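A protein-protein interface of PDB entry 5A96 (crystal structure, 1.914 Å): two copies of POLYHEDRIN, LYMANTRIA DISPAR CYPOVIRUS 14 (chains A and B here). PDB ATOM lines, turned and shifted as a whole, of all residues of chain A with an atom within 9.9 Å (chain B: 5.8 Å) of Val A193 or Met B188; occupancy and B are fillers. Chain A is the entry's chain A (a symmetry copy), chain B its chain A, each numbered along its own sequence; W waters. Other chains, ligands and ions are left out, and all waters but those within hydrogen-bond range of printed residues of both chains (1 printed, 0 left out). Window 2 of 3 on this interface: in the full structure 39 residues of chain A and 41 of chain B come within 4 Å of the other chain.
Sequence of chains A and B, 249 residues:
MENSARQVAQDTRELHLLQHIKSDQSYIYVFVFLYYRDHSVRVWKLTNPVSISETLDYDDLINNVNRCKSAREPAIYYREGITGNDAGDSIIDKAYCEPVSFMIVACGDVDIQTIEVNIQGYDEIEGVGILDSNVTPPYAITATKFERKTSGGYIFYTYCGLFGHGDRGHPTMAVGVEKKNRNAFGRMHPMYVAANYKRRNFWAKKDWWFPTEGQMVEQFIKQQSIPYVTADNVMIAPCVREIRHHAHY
Pro B190 touches its own counterpart, Pro A190.
Val A193 touches Met B188, but with the chains exchanged Met A188 does not touch Val B193 (6.6 Å).
Tyr A197 touches Met B188, but with the chains exchanged Met A188 does not touch Tyr B197 (6.7 Å).
Tyr A197 touches Asn B196, but with the chains exchanged Asn A196 does not touch Tyr B197 (9.5 Å).
10 positions are printed for both chains.
Of the 5 pairs that touch across the chains among the printed residues, 2 have their exchanged pair printed and touching as well.
The backbone carbonyl oxygen (O) of Asn B196 sits at hydrogen-bond distance from the side-chain hydroxyl (OH) of Tyr A197, 3.2 Å away.
Printed residues of chain B that touch a printed residue of chain A: Met B188, Pro B190, Asn B196 and Tyr B197.
Hydrophobic or aromatic side chains of chain A that line the printed part of chain B: Pro A190, Val A193 and Tyr A197.
Along chain A the printed residues that touch a printed residue of chain B span positions 190 to 197.
Among the printed residues, no Asp or Glu carboxylate lies within 4 Å of a Lys or Arg side-chain nitrogen of the other chain.
CG of Pro A190 touches CG of Pro B190 (3.7 Å).
CG1 of Val A193 touches O of Met B188, at 3.6 Å.
CD2 of Tyr A197 touches CE of Met B188, 3.6 Å away.
Tyr A197 touches Tyr B197.
ND2 of Asn B196 lies within hydrogen-bond range of O of Arg B187.
The guanidinium group (NH1) of Arg A200 sits at hydrogen-bond distance from the backbone carbonyl oxygen (O) of Tyr A197 (2.9 Å).
Of the printed residues of chain B, Val A193 touches Met B188.
Met B188 touches two residues of chain A.
Of chain A, only Tyr A197 comes within 4 Å of Asn B196.
Of the printed residues of chain A, Pro B190 touches Pro A190 (3.7 Å).
Printed residues of chain B within 4 Å of Pro A190: Pro B190 (3.7 Å).
Printed residues of chain B within 4 Å of Tyr A197: Met B188 (3.6 Å), Asn B196 (3.2 Å) and Tyr B197 (3.7 Å).
Printed residues of chain A within 4 Å of Tyr B197: Tyr A197.
His A189 touches none of the printed residues of chain B.
Asn A48 touches none of the printed residues of chain B.
The nearest residue of chain B that does not touch Val A193 is Val B193 (5.0 Å).
Water W1 bridges O of Asn B196 and OH of Tyr A197.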
ATOM      1  N   ASN A  48     -17.510  -1.478 -33.572  1.00  0.00           N
ATOM      2  CA  ASN A  48     -16.431  -0.546 -33.344  1.00  0.00           C
ATOM      3  C   ASN A  48     -15.511  -1.110 -32.270  1.00  0.00           C
ATOM      4  O   ASN A  48     -15.928  -1.949 -31.472  1.00  0.00           O
ATOM      5  CB  ASN A  48     -16.993   0.816 -32.908  1.00  0.00           C
ATOM      6  CG  ASN A  48     -15.968   1.923 -33.001  1.00  0.00           C
ATOM      7  OD1 ASN A  48     -15.280   2.246 -32.025  1.00  0.00           O
ATOM      8  ND2 ASN A  48     -15.842   2.501 -34.185  1.00  0.00           N
ATOM      9  N   VAL A  50     -14.475   0.609 -29.683  1.00  0.00           N
ATOM     10  CA  VAL A  50     -14.759   1.215 -28.382  1.00  0.00           C
ATOM     11  C   VAL A  50     -16.109   1.929 -28.318  1.00  0.00           C
ATOM     12  O   VAL A  50     -16.684   2.084 -27.235  1.00  0.00           O
ATOM     13  CB  VAL A  50     -13.634   2.229 -27.980  1.00  0.00           C
ATOM     14  CG1 VAL A  50     -12.260   1.545 -27.978  1.00  0.00           C
ATOM     15  CG2 VAL A  50     -13.619   3.427 -28.922  1.00  0.00           C
ATOM     16  N   SER A  51     -16.632   2.360 -29.465  1.00  0.00           N
ATOM     17  CA  SER A  51     -17.831   3.201 -29.467  1.00  0.00           C
ATOM     18  C   SER A  51     -18.646   3.062 -30.755  1.00  0.00           C
ATOM     19  O   SER A  51     -18.238   3.526 -31.822  1.00  0.00           O
ATOM     20  CB  SER A  51     -17.435   4.668 -29.276  1.00  0.00           C
ATOM     21  OG  SER A  51     -18.576   5.517 -29.251  1.00  0.00           O
ATOM     22  N   PHE A 185      -8.891   4.504 -16.817  1.00  0.00           N
ATOM     23  CA  PHE A 185      -8.298   5.152 -18.001  1.00  0.00           C
ATOM     24  C   PHE A 185      -9.246   5.078 -19.193  1.00  0.00           C
ATOM     25  O   PHE A 185      -9.465   4.013 -19.770  1.00  0.00           O
ATOM     26  CB  PHE A 185      -6.930   4.549 -18.349  1.00  0.00           C
ATOM     27  CG  PHE A 185      -6.242   5.236 -19.502  1.00  0.00           C
ATOM     28  CD1 PHE A 185      -5.776   6.545 -19.376  1.00  0.00           C
ATOM     29  CD2 PHE A 185      -6.075   4.582 -20.719  1.00  0.00           C
ATOM     30  CE1 PHE A 185      -5.140   7.180 -20.445  1.00  0.00           C
ATOM     31  CE2 PHE A 185      -5.443   5.214 -21.792  1.00  0.00           C
ATOM     32  CZ  PHE A 185      -4.982   6.518 -21.648  1.00  0.00           C
ATOM     33  N   GLY A 186      -9.823   6.224 -19.540  1.00  0.00           N
ATOM     34  CA  GLY A 186     -10.843   6.293 -20.565  1.00  0.00           C
ATOM     35  C   GLY A 186     -10.296   5.956 -21.938  1.00  0.00           C
ATOM     36  O   GLY A 186      -9.194   6.356 -22.298  1.00  0.00           O
ATOM     37  N   ARG A 187     -11.076   5.218 -22.717  1.00  0.00           N
ATOM     38  CA  ARG A 187     -10.675   4.901 -24.076  1.00  0.00           C
ATOM     39  C   ARG A 187     -10.651   6.165 -24.941  1.00  0.00           C
ATOM     40  O   ARG A 187     -10.059   6.166 -26.016  1.00  0.00           O
ATOM     41  CB  ARG A 187     -11.572   3.799 -24.637  1.00  0.00           C
ATOM     42  CG  ARG A 187     -11.508   2.565 -23.728  1.00  0.00           C
ATOM     43  CD  ARG A 187     -11.355   1.250 -24.478  1.00  0.00           C
ATOM     44  NE  ARG A 187     -10.955   0.168 -23.571  1.00  0.00           N
ATOM     45  CZ  ARG A 187     -11.725  -0.352 -22.613  1.00  0.00           C
ATOM     46  NH1 ARG A 187     -12.956   0.094 -22.409  1.00  0.00           N
ATOM     47  NH2 ARG A 187     -11.261  -1.331 -21.856  1.00  0.00           N
ATOM     48  N   MET A 188     -11.259   7.248 -24.461  1.00  0.00           N
ATOM     49  CA  MET A 188     -11.136   8.551 -25.131  1.00  0.00           C
ATOM     50  C   MET A 188     -10.403   9.600 -24.262  1.00  0.00           C
ATOM     51  O   MET A 188     -10.556  10.816 -24.460  1.00  0.00           O
ATOM     52  CB  MET A 188     -12.516   9.070 -25.575  1.00  0.00           C
ATOM     53  CG  MET A 188     -13.208   8.197 -26.626  1.00  0.00           C
ATOM     54  SD  MET A 188     -12.289   8.101 -28.171  1.00  0.00           S
ATOM     55  CE  MET A 188     -12.885   9.589 -29.009  1.00  0.00           C
ATOM     56  N   HIS A 189      -9.601   9.132 -23.306  1.00  0.00           N
ATOM     57  CA  HIS A 189      -8.668  10.004 -22.581  1.00  0.00           C
ATOM     58  C   HIS A 189      -7.693  10.618 -23.595  1.00  0.00           C
ATOM     59  O   HIS A 189      -7.383   9.985 -24.585  1.00  0.00           O
ATOM     60  CB  HIS A 189      -7.899   9.179 -21.540  1.00  0.00           C
ATOM     61  CG  HIS A 189      -7.009   9.995 -20.656  1.00  0.00           C
ATOM     62  ND1 HIS A 189      -5.708  10.307 -20.989  1.00  0.00           N
ATOM     63  CD2 HIS A 189      -7.232  10.559 -19.445  1.00  0.00           C
ATOM     64  CE1 HIS A 189      -5.171  11.036 -20.026  1.00  0.00           C
ATOM     65  NE2 HIS A 189      -6.076  11.201 -19.077  1.00  0.00           N
ATOM     66  N   PRO A 190      -7.202  11.847 -23.355  1.00  0.00           N
ATOM     67  CA  PRO A 190      -6.297  12.503 -24.312  1.00  0.00           C
ATOM     68  C   PRO A 190      -5.110  11.659 -24.817  1.00  0.00           C
ATOM     69  O   PRO A 190      -4.653  11.876 -25.934  1.00  0.00           O
ATOM     70  CB  PRO A 190      -5.782  13.712 -23.517  1.00  0.00           C
ATOM     71  CG  PRO A 190      -6.930  14.055 -22.603  1.00  0.00           C
ATOM     72  CD  PRO A 190      -7.532  12.729 -22.221  1.00  0.00           C
ATOM     73  N   MET A 191      -4.617  10.731 -24.004  1.00  0.00           N
ATOM     74  CA  MET A 191      -3.497   9.874 -24.400  1.00  0.00           C
ATOM     75  C   MET A 191      -3.925   8.709 -25.296  1.00  0.00           C
ATOM     76  O   MET A 191      -3.092   8.005 -25.857  1.00  0.00           O
ATOM     77  CB  MET A 191      -2.785   9.330 -23.167  1.00  0.00           C
ATOM     78  CG  MET A 191      -1.932  10.357 -22.448  1.00  0.00           C
ATOM     79  SD  MET A 191      -1.031   9.642 -21.066  1.00  0.00           S
ATOM     80  CE  MET A 191      -0.030  11.049 -20.596  1.00  0.00           C
ATOM     81  N   TYR A 192      -5.231   8.500 -25.390  1.00  0.00           N
ATOM     82  CA  TYR A 192      -5.801   7.381 -26.151  1.00  0.00           C
ATOM     83  C   TYR A 192      -6.674   7.866 -27.321  1.00  0.00           C
ATOM     84  O   TYR A 192      -6.809   7.183 -28.346  1.00  0.00           O
ATOM     85  CB  TYR A 192      -6.662   6.525 -25.213  1.00  0.00           C
ATOM     86  CG  TYR A 192      -6.741   5.053 -25.563  1.00  0.00           C
ATOM     87  CD1 TYR A 192      -6.277   4.569 -26.783  1.00  0.00           C
ATOM     88  CD2 TYR A 192      -7.273   4.144 -24.660  1.00  0.00           C
ATOM     89  CE1 TYR A 192      -6.351   3.223 -27.093  1.00  0.00           C
ATOM     90  CE2 TYR A 192      -7.353   2.801 -24.961  1.00  0.00           C
ATOM     91  CZ  TYR A 192      -6.888   2.346 -26.174  1.00  0.00           C
ATOM     92  OH  TYR A 192      -6.965   1.003 -26.463  1.00  0.00           O
ATOM     93  N   VAL A 193      -7.255   9.055 -27.158  1.00  0.00           N
ATOM     94  CA  VAL A 193      -8.368   9.521 -27.984  1.00  0.00           C
ATOM     95  C   VAL A 193      -8.069   9.457 -29.481  1.00  0.00           C
ATOM     96  O   VAL A 193      -8.863   8.923 -30.252  1.00  0.00           O
ATOM     97  CB  VAL A 193      -8.798  10.966 -27.568  1.00  0.00           C
ATOM     98  CG1 VAL A 193      -7.621  11.940 -27.671  1.00  0.00           C
ATOM     99  CG2 VAL A 193      -9.982  11.456 -28.389  1.00  0.00           C
ATOM    100  N   ALA A 194      -6.922   9.978 -29.893  1.00  0.00           N
ATOM    101  CA  ALA A 194      -6.579  10.012 -31.314  1.00  0.00           C
ATOM    102  C   ALA A 194      -6.548   8.630 -31.966  1.00  0.00           C
ATOM    103  O   ALA A 194      -6.872   8.502 -33.149  1.00  0.00           O
ATOM    104  CB  ALA A 194      -5.237  10.718 -31.530  1.00  0.00           C
ATOM    105  N   ALA A 195      -6.136   7.605 -31.216  1.00  0.00           N
ATOM    106  CA  ALA A 195      -6.044   6.256 -31.774  1.00  0.00           C
ATOM    107  C   ALA A 195      -7.421   5.629 -31.965  1.00  0.00           C
ATOM    108  O   ALA A 195      -7.615   4.796 -32.847  1.00  0.00           O
ATOM    109  CB  ALA A 195      -5.175   5.370 -30.899  1.00  0.00           C
ATOM    110  N   ASN A 196      -8.377   6.017 -31.138  1.00  0.00           N
ATOM    111  CA  ASN A 196      -9.729   5.495 -31.275  1.00  0.00           C
ATOM    112  C   ASN A 196     -10.568   6.320 -32.254  1.00  0.00           C
ATOM    113  O   ASN A 196     -11.429   5.799 -32.963  1.00  0.00           O
ATOM    114  CB  ASN A 196     -10.375   5.393 -29.900  1.00  0.00           C
ATOM    115  CG  ASN A 196      -9.856   4.196 -29.121  1.00  0.00           C
ATOM    116  OD1 ASN A 196      -9.654   3.125 -29.675  1.00  0.00           O
ATOM    117  ND2 ASN A 196      -9.607   4.386 -27.853  1.00  0.00           N
ATOM    118  N   TYR A 197     -10.284   7.609 -32.304  1.00  0.00           N
ATOM    119  CA  TYR A 197     -10.901   8.509 -33.269  1.00  0.00           C
ATOM    120  C   TYR A 197     -10.560   8.092 -34.690  1.00  0.00           C
ATOM    121  O   TYR A 197     -11.380   8.213 -35.595  1.00  0.00           O
ATOM    122  CB  TYR A 197     -10.394   9.924 -33.014  1.00  0.00           C
ATOM    123  CG  TYR A 197     -11.071  10.996 -33.832  1.00  0.00           C
ATOM    124  CD1 TYR A 197     -12.455  11.133 -33.830  1.00  0.00           C
ATOM    125  CD2 TYR A 197     -10.316  11.907 -34.573  1.00  0.00           C
ATOM    126  CE1 TYR A 197     -13.068  12.124 -34.558  1.00  0.00           C
ATOM    127  CE2 TYR A 197     -10.917  12.905 -35.304  1.00  0.00           C
ATOM    128  CZ  TYR A 197     -12.286  13.011 -35.293  1.00  0.00           C
ATOM    129  OH  TYR A 197     -12.875  14.016 -36.002  1.00  0.00           O
ATOM    130  N   LYS A 198      -9.333   7.613 -34.875  1.00  0.00           N
ATOM    131  CA  LYS A 198      -8.881   7.123 -36.167  1.00  0.00           C
ATOM    132  C   LYS A 198      -9.713   5.912 -36.604  1.00  0.00           C
ATOM    133  O   LYS A 198      -9.727   5.538 -37.784  1.00  0.00           O
ATOM    134  CB  LYS A 198      -7.413   6.708 -36.060  1.00  0.00           C
ATOM    135  CG  LYS A 198      -6.692   6.636 -37.393  1.00  0.00           C
ATOM    136  CD  LYS A 198      -5.414   5.846 -37.272  1.00  0.00           C
ATOM    137  CE  LYS A 198      -5.692   4.357 -37.158  1.00  0.00           C
ATOM    138  NZ  LYS A 198      -4.470   3.662 -36.702  1.00  0.00           N
ATOM    139  N   ARG A 199     -10.379   5.285 -35.639  1.00  0.00           N
ATOM    140  CA  ARG A 199     -11.139   4.068 -35.902  1.00  0.00           C
ATOM    141  C   ARG A 199     -12.634   4.256 -35.679  1.00  0.00           C
ATOM    142  O   ARG A 199     -13.375   3.287 -35.432  1.00  0.00           O
ATOM    143  CB  ARG A 199     -10.607   2.926 -35.039  1.00  0.00           C
ATOM    144  CG  ARG A 199      -9.118   2.688 -35.229  1.00  0.00           C
ATOM    145  CD  ARG A 199      -8.639   1.453 -34.498  1.00  0.00           C
ATOM    146  NE  ARG A 199      -8.671   1.628 -33.051  1.00  0.00           N
ATOM    147  CZ  ARG A 199      -8.340   0.678 -32.179  1.00  0.00           C
ATOM    148  NH1 ARG A 199      -7.968  -0.530 -32.602  1.00  0.00           N
ATOM    149  NH2 ARG A 199      -8.381   0.934 -30.877  1.00  0.00           N
ATOM    150  N   ARG A 200     -13.080   5.505 -35.773  1.00  0.00           N
ATOM    151  CA  ARG A 200     -14.499   5.832 -35.596  1.00  0.00           C
ATOM    152  C   ARG A 200     -15.395   5.203 -36.662  1.00  0.00           C
ATOM    153  O   ARG A 200     -16.578   4.979 -36.413  1.00  0.00           O
ATOM    154  CB  ARG A 200     -14.697   7.344 -35.595  1.00  0.00           C
ATOM    155  CG  ARG A 200     -14.446   8.028 -36.948  1.00  0.00           C
ATOM    156  CD  ARG A 200     -14.414   9.541 -36.739  1.00  0.00           C
ATOM    157  NE  ARG A 200     -14.073  10.312 -37.932  1.00  0.00           N
ATOM    158  CZ  ARG A 200     -12.840  10.668 -38.288  1.00  0.00           C
ATOM    159  NH1 ARG A 200     -11.782  10.305 -37.562  1.00  0.00           N
ATOM    160  NH2 ARG A 200     -12.669  11.393 -39.385  1.00  0.00           N
ATOM    161  N   VAL B  50      -7.174  16.041 -39.956  1.00  0.00           N
ATOM    162  CA  VAL B  50      -6.291  15.449 -38.950  1.00  0.00           C
ATOM    163  C   VAL B  50      -6.424  13.931 -38.834  1.00  0.00           C
ATOM    164  O   VAL B  50      -5.487  13.253 -38.398  1.00  0.00           O
ATOM    165  CB  VAL B  50      -6.545  16.086 -37.541  1.00  0.00           C
ATOM    166  CG1 VAL B  50      -6.371  17.610 -37.593  1.00  0.00           C
ATOM    167  CG2 VAL B  50      -7.936  15.735 -37.027  1.00  0.00           C
ATOM    168  N   GLY B 186      -1.478  17.459 -28.929  1.00  0.00           N
ATOM    169  CA  GLY B 186      -2.294  16.573 -29.732  1.00  0.00           C
ATOM    170  C   GLY B 186      -3.395  17.315 -30.462  1.00  0.00           C
ATOM    171  O   GLY B 186      -4.022  18.218 -29.917  1.00  0.00           O
ATOM    172  N   ARG B 187      -3.641  16.927 -31.707  1.00  0.00           N
ATOM    173  CA  ARG B 187      -4.723  17.526 -32.467  1.00  0.00           C
ATOM    174  C   ARG B 187      -6.080  17.154 -31.861  1.00  0.00           C
ATOM    175  O   ARG B 187      -7.086  17.789 -32.161  1.00  0.00           O
ATOM    176  CB  ARG B 187      -4.593  17.146 -33.940  1.00  0.00           C
ATOM    177  CG  ARG B 187      -3.222  17.585 -34.471  1.00  0.00           C
ATOM    178  CD  ARG B 187      -3.274  18.272 -35.828  1.00  0.00           C
ATOM    179  NE  ARG B 187      -2.014  18.967 -36.115  1.00  0.00           N
ATOM    180  CZ  ARG B 187      -0.844  18.367 -36.350  1.00  0.00           C
ATOM    181  NH1 ARG B 187      -0.740  17.045 -36.339  1.00  0.00           N
ATOM    182  NH2 ARG B 187       0.229  19.095 -36.604  1.00  0.00           N
ATOM    183  N   MET B 188      -6.105  16.153 -30.982  1.00  0.00           N
ATOM    184  CA  MET B 188      -7.320  15.842 -30.215  1.00  0.00           C
ATOM    185  C   MET B 188      -7.139  16.065 -28.695  1.00  0.00           C
ATOM    186  O   MET B 188      -7.869  15.492 -27.872  1.00  0.00           O
ATOM    187  CB  MET B 188      -7.801  14.409 -30.509  1.00  0.00           C
ATOM    188  CG  MET B 188      -8.230  14.175 -31.961  1.00  0.00           C
ATOM    189  SD  MET B 188      -9.638  15.187 -32.447  1.00  0.00           S
ATOM    190  CE  MET B 188     -11.007  14.156 -31.871  1.00  0.00           C
ATOM    191  N   HIS B 189      -6.170  16.902 -28.324  1.00  0.00           N
ATOM    192  CA  HIS B 189      -6.052  17.386 -26.943  1.00  0.00           C
ATOM    193  C   HIS B 189      -7.337  18.146 -26.585  1.00  0.00           C
ATOM    194  O   HIS B 189      -7.938  18.747 -27.454  1.00  0.00           O
ATOM    195  CB  HIS B 189      -4.838  18.317 -26.828  1.00  0.00           C
ATOM    196  CG  HIS B 189      -4.550  18.770 -25.431  1.00  0.00           C
ATOM    197  ND1 HIS B 189      -5.132  19.888 -24.872  1.00  0.00           N
ATOM    198  CD2 HIS B 189      -3.733  18.258 -24.480  1.00  0.00           C
ATOM    199  CE1 HIS B 189      -4.695  20.038 -23.634  1.00  0.00           C
ATOM    200  NE2 HIS B 189      -3.843  19.062 -23.373  1.00  0.00           N
ATOM    201  N   PRO B 190      -7.763  18.129 -25.309  1.00  0.00           N
ATOM    202  CA  PRO B 190      -9.010  18.804 -24.916  1.00  0.00           C
ATOM    203  C   PRO B 190      -9.184  20.255 -25.408  1.00  0.00           C
ATOM    204  O   PRO B 190     -10.314  20.689 -25.603  1.00  0.00           O
ATOM    205  CB  PRO B 190      -8.944  18.772 -23.383  1.00  0.00           C
ATOM    206  CG  PRO B 190      -8.180  17.508 -23.084  1.00  0.00           C
ATOM    207  CD  PRO B 190      -7.152  17.407 -24.179  1.00  0.00           C
ATOM    208  N   TYR B 192      -8.177  21.352 -28.254  1.00  0.00           N
ATOM    209  CA  TYR B 192      -8.251  21.297 -29.720  1.00  0.00           C
ATOM    210  C   TYR B 192      -9.406  20.406 -30.205  1.00  0.00           C
ATOM    211  O   TYR B 192      -9.964  20.616 -31.292  1.00  0.00           O
ATOM    212  CB  TYR B 192      -6.931  20.738 -30.266  1.00  0.00           C
ATOM    213  CG  TYR B 192      -6.532  21.235 -31.641  1.00  0.00           C
ATOM    214  CD1 TYR B 192      -7.421  21.942 -32.445  1.00  0.00           C
ATOM    215  CD2 TYR B 192      -5.253  21.004 -32.128  1.00  0.00           C
ATOM    216  CE1 TYR B 192      -7.047  22.394 -33.698  1.00  0.00           C
ATOM    217  CE2 TYR B 192      -4.873  21.448 -33.376  1.00  0.00           C
ATOM    218  CZ  TYR B 192      -5.770  22.145 -34.154  1.00  0.00           C
ATOM    219  OH  TYR B 192      -5.378  22.591 -35.395  1.00  0.00           O
ATOM    220  N   VAL B 193      -9.762  19.417 -29.385  1.00  0.00           N
ATOM    221  CA  VAL B 193     -10.580  18.281 -29.809  1.00  0.00           C
ATOM    222  C   VAL B 193     -11.891  18.704 -30.468  1.00  0.00           C
ATOM    223  O   VAL B 193     -12.225  18.227 -31.552  1.00  0.00           O
ATOM    224  CB  VAL B 193     -10.852  17.318 -28.607  1.00  0.00           C
ATOM    225  CG1 VAL B 193     -11.533  18.058 -27.453  1.00  0.00           C
ATOM    226  CG2 VAL B 193     -11.670  16.108 -29.034  1.00  0.00           C
ATOM    227  N   ASN B 196     -11.679  19.819 -34.127  1.00  0.00           N
ATOM    228  CA  ASN B 196     -11.402  18.770 -35.097  1.00  0.00           C
ATOM    229  C   ASN B 196     -12.555  17.769 -35.208  1.00  0.00           C
ATOM    230  O   ASN B 196     -12.833  17.220 -36.274  1.00  0.00           O
ATOM    231  CB  ASN B 196     -10.081  18.097 -34.754  1.00  0.00           C
ATOM    232  CG  ASN B 196      -8.891  18.954 -35.152  1.00  0.00           C
ATOM    233  OD1 ASN B 196      -8.892  19.581 -36.203  1.00  0.00           O
ATOM    234  ND2 ASN B 196      -7.901  19.012 -34.303  1.00  0.00           N
ATOM    235  N   TYR B 197     -13.240  17.562 -34.098  1.00  0.00           N
ATOM    236  CA  TYR B 197     -14.440  16.737 -34.062  1.00  0.00           C
ATOM    237  C   TYR B 197     -15.524  17.323 -34.953  1.00  0.00           C
ATOM    238  O   TYR B 197     -16.281  16.592 -35.584  1.00  0.00           O
ATOM    239  CB  TYR B 197     -14.943  16.666 -32.623  1.00  0.00           C
ATOM    240  CG  TYR B 197     -16.090  15.711 -32.400  1.00  0.00           C
ATOM    241  CD1 TYR B 197     -15.999  14.378 -32.788  1.00  0.00           C
ATOM    242  CD2 TYR B 197     -17.252  16.136 -31.754  1.00  0.00           C
ATOM    243  CE1 TYR B 197     -17.036  13.506 -32.564  1.00  0.00           C
ATOM    244  CE2 TYR B 197     -18.296  15.272 -31.521  1.00  0.00           C
ATOM    245  CZ  TYR B 197     -18.185  13.963 -31.924  1.00  0.00           C
ATOM    246  OH  TYR B 197     -19.215  13.106 -31.671  1.00  0.00           O
HETATM  247  O   HOH W   1     -11.373  15.474 -37.665  1.00  0.00           O
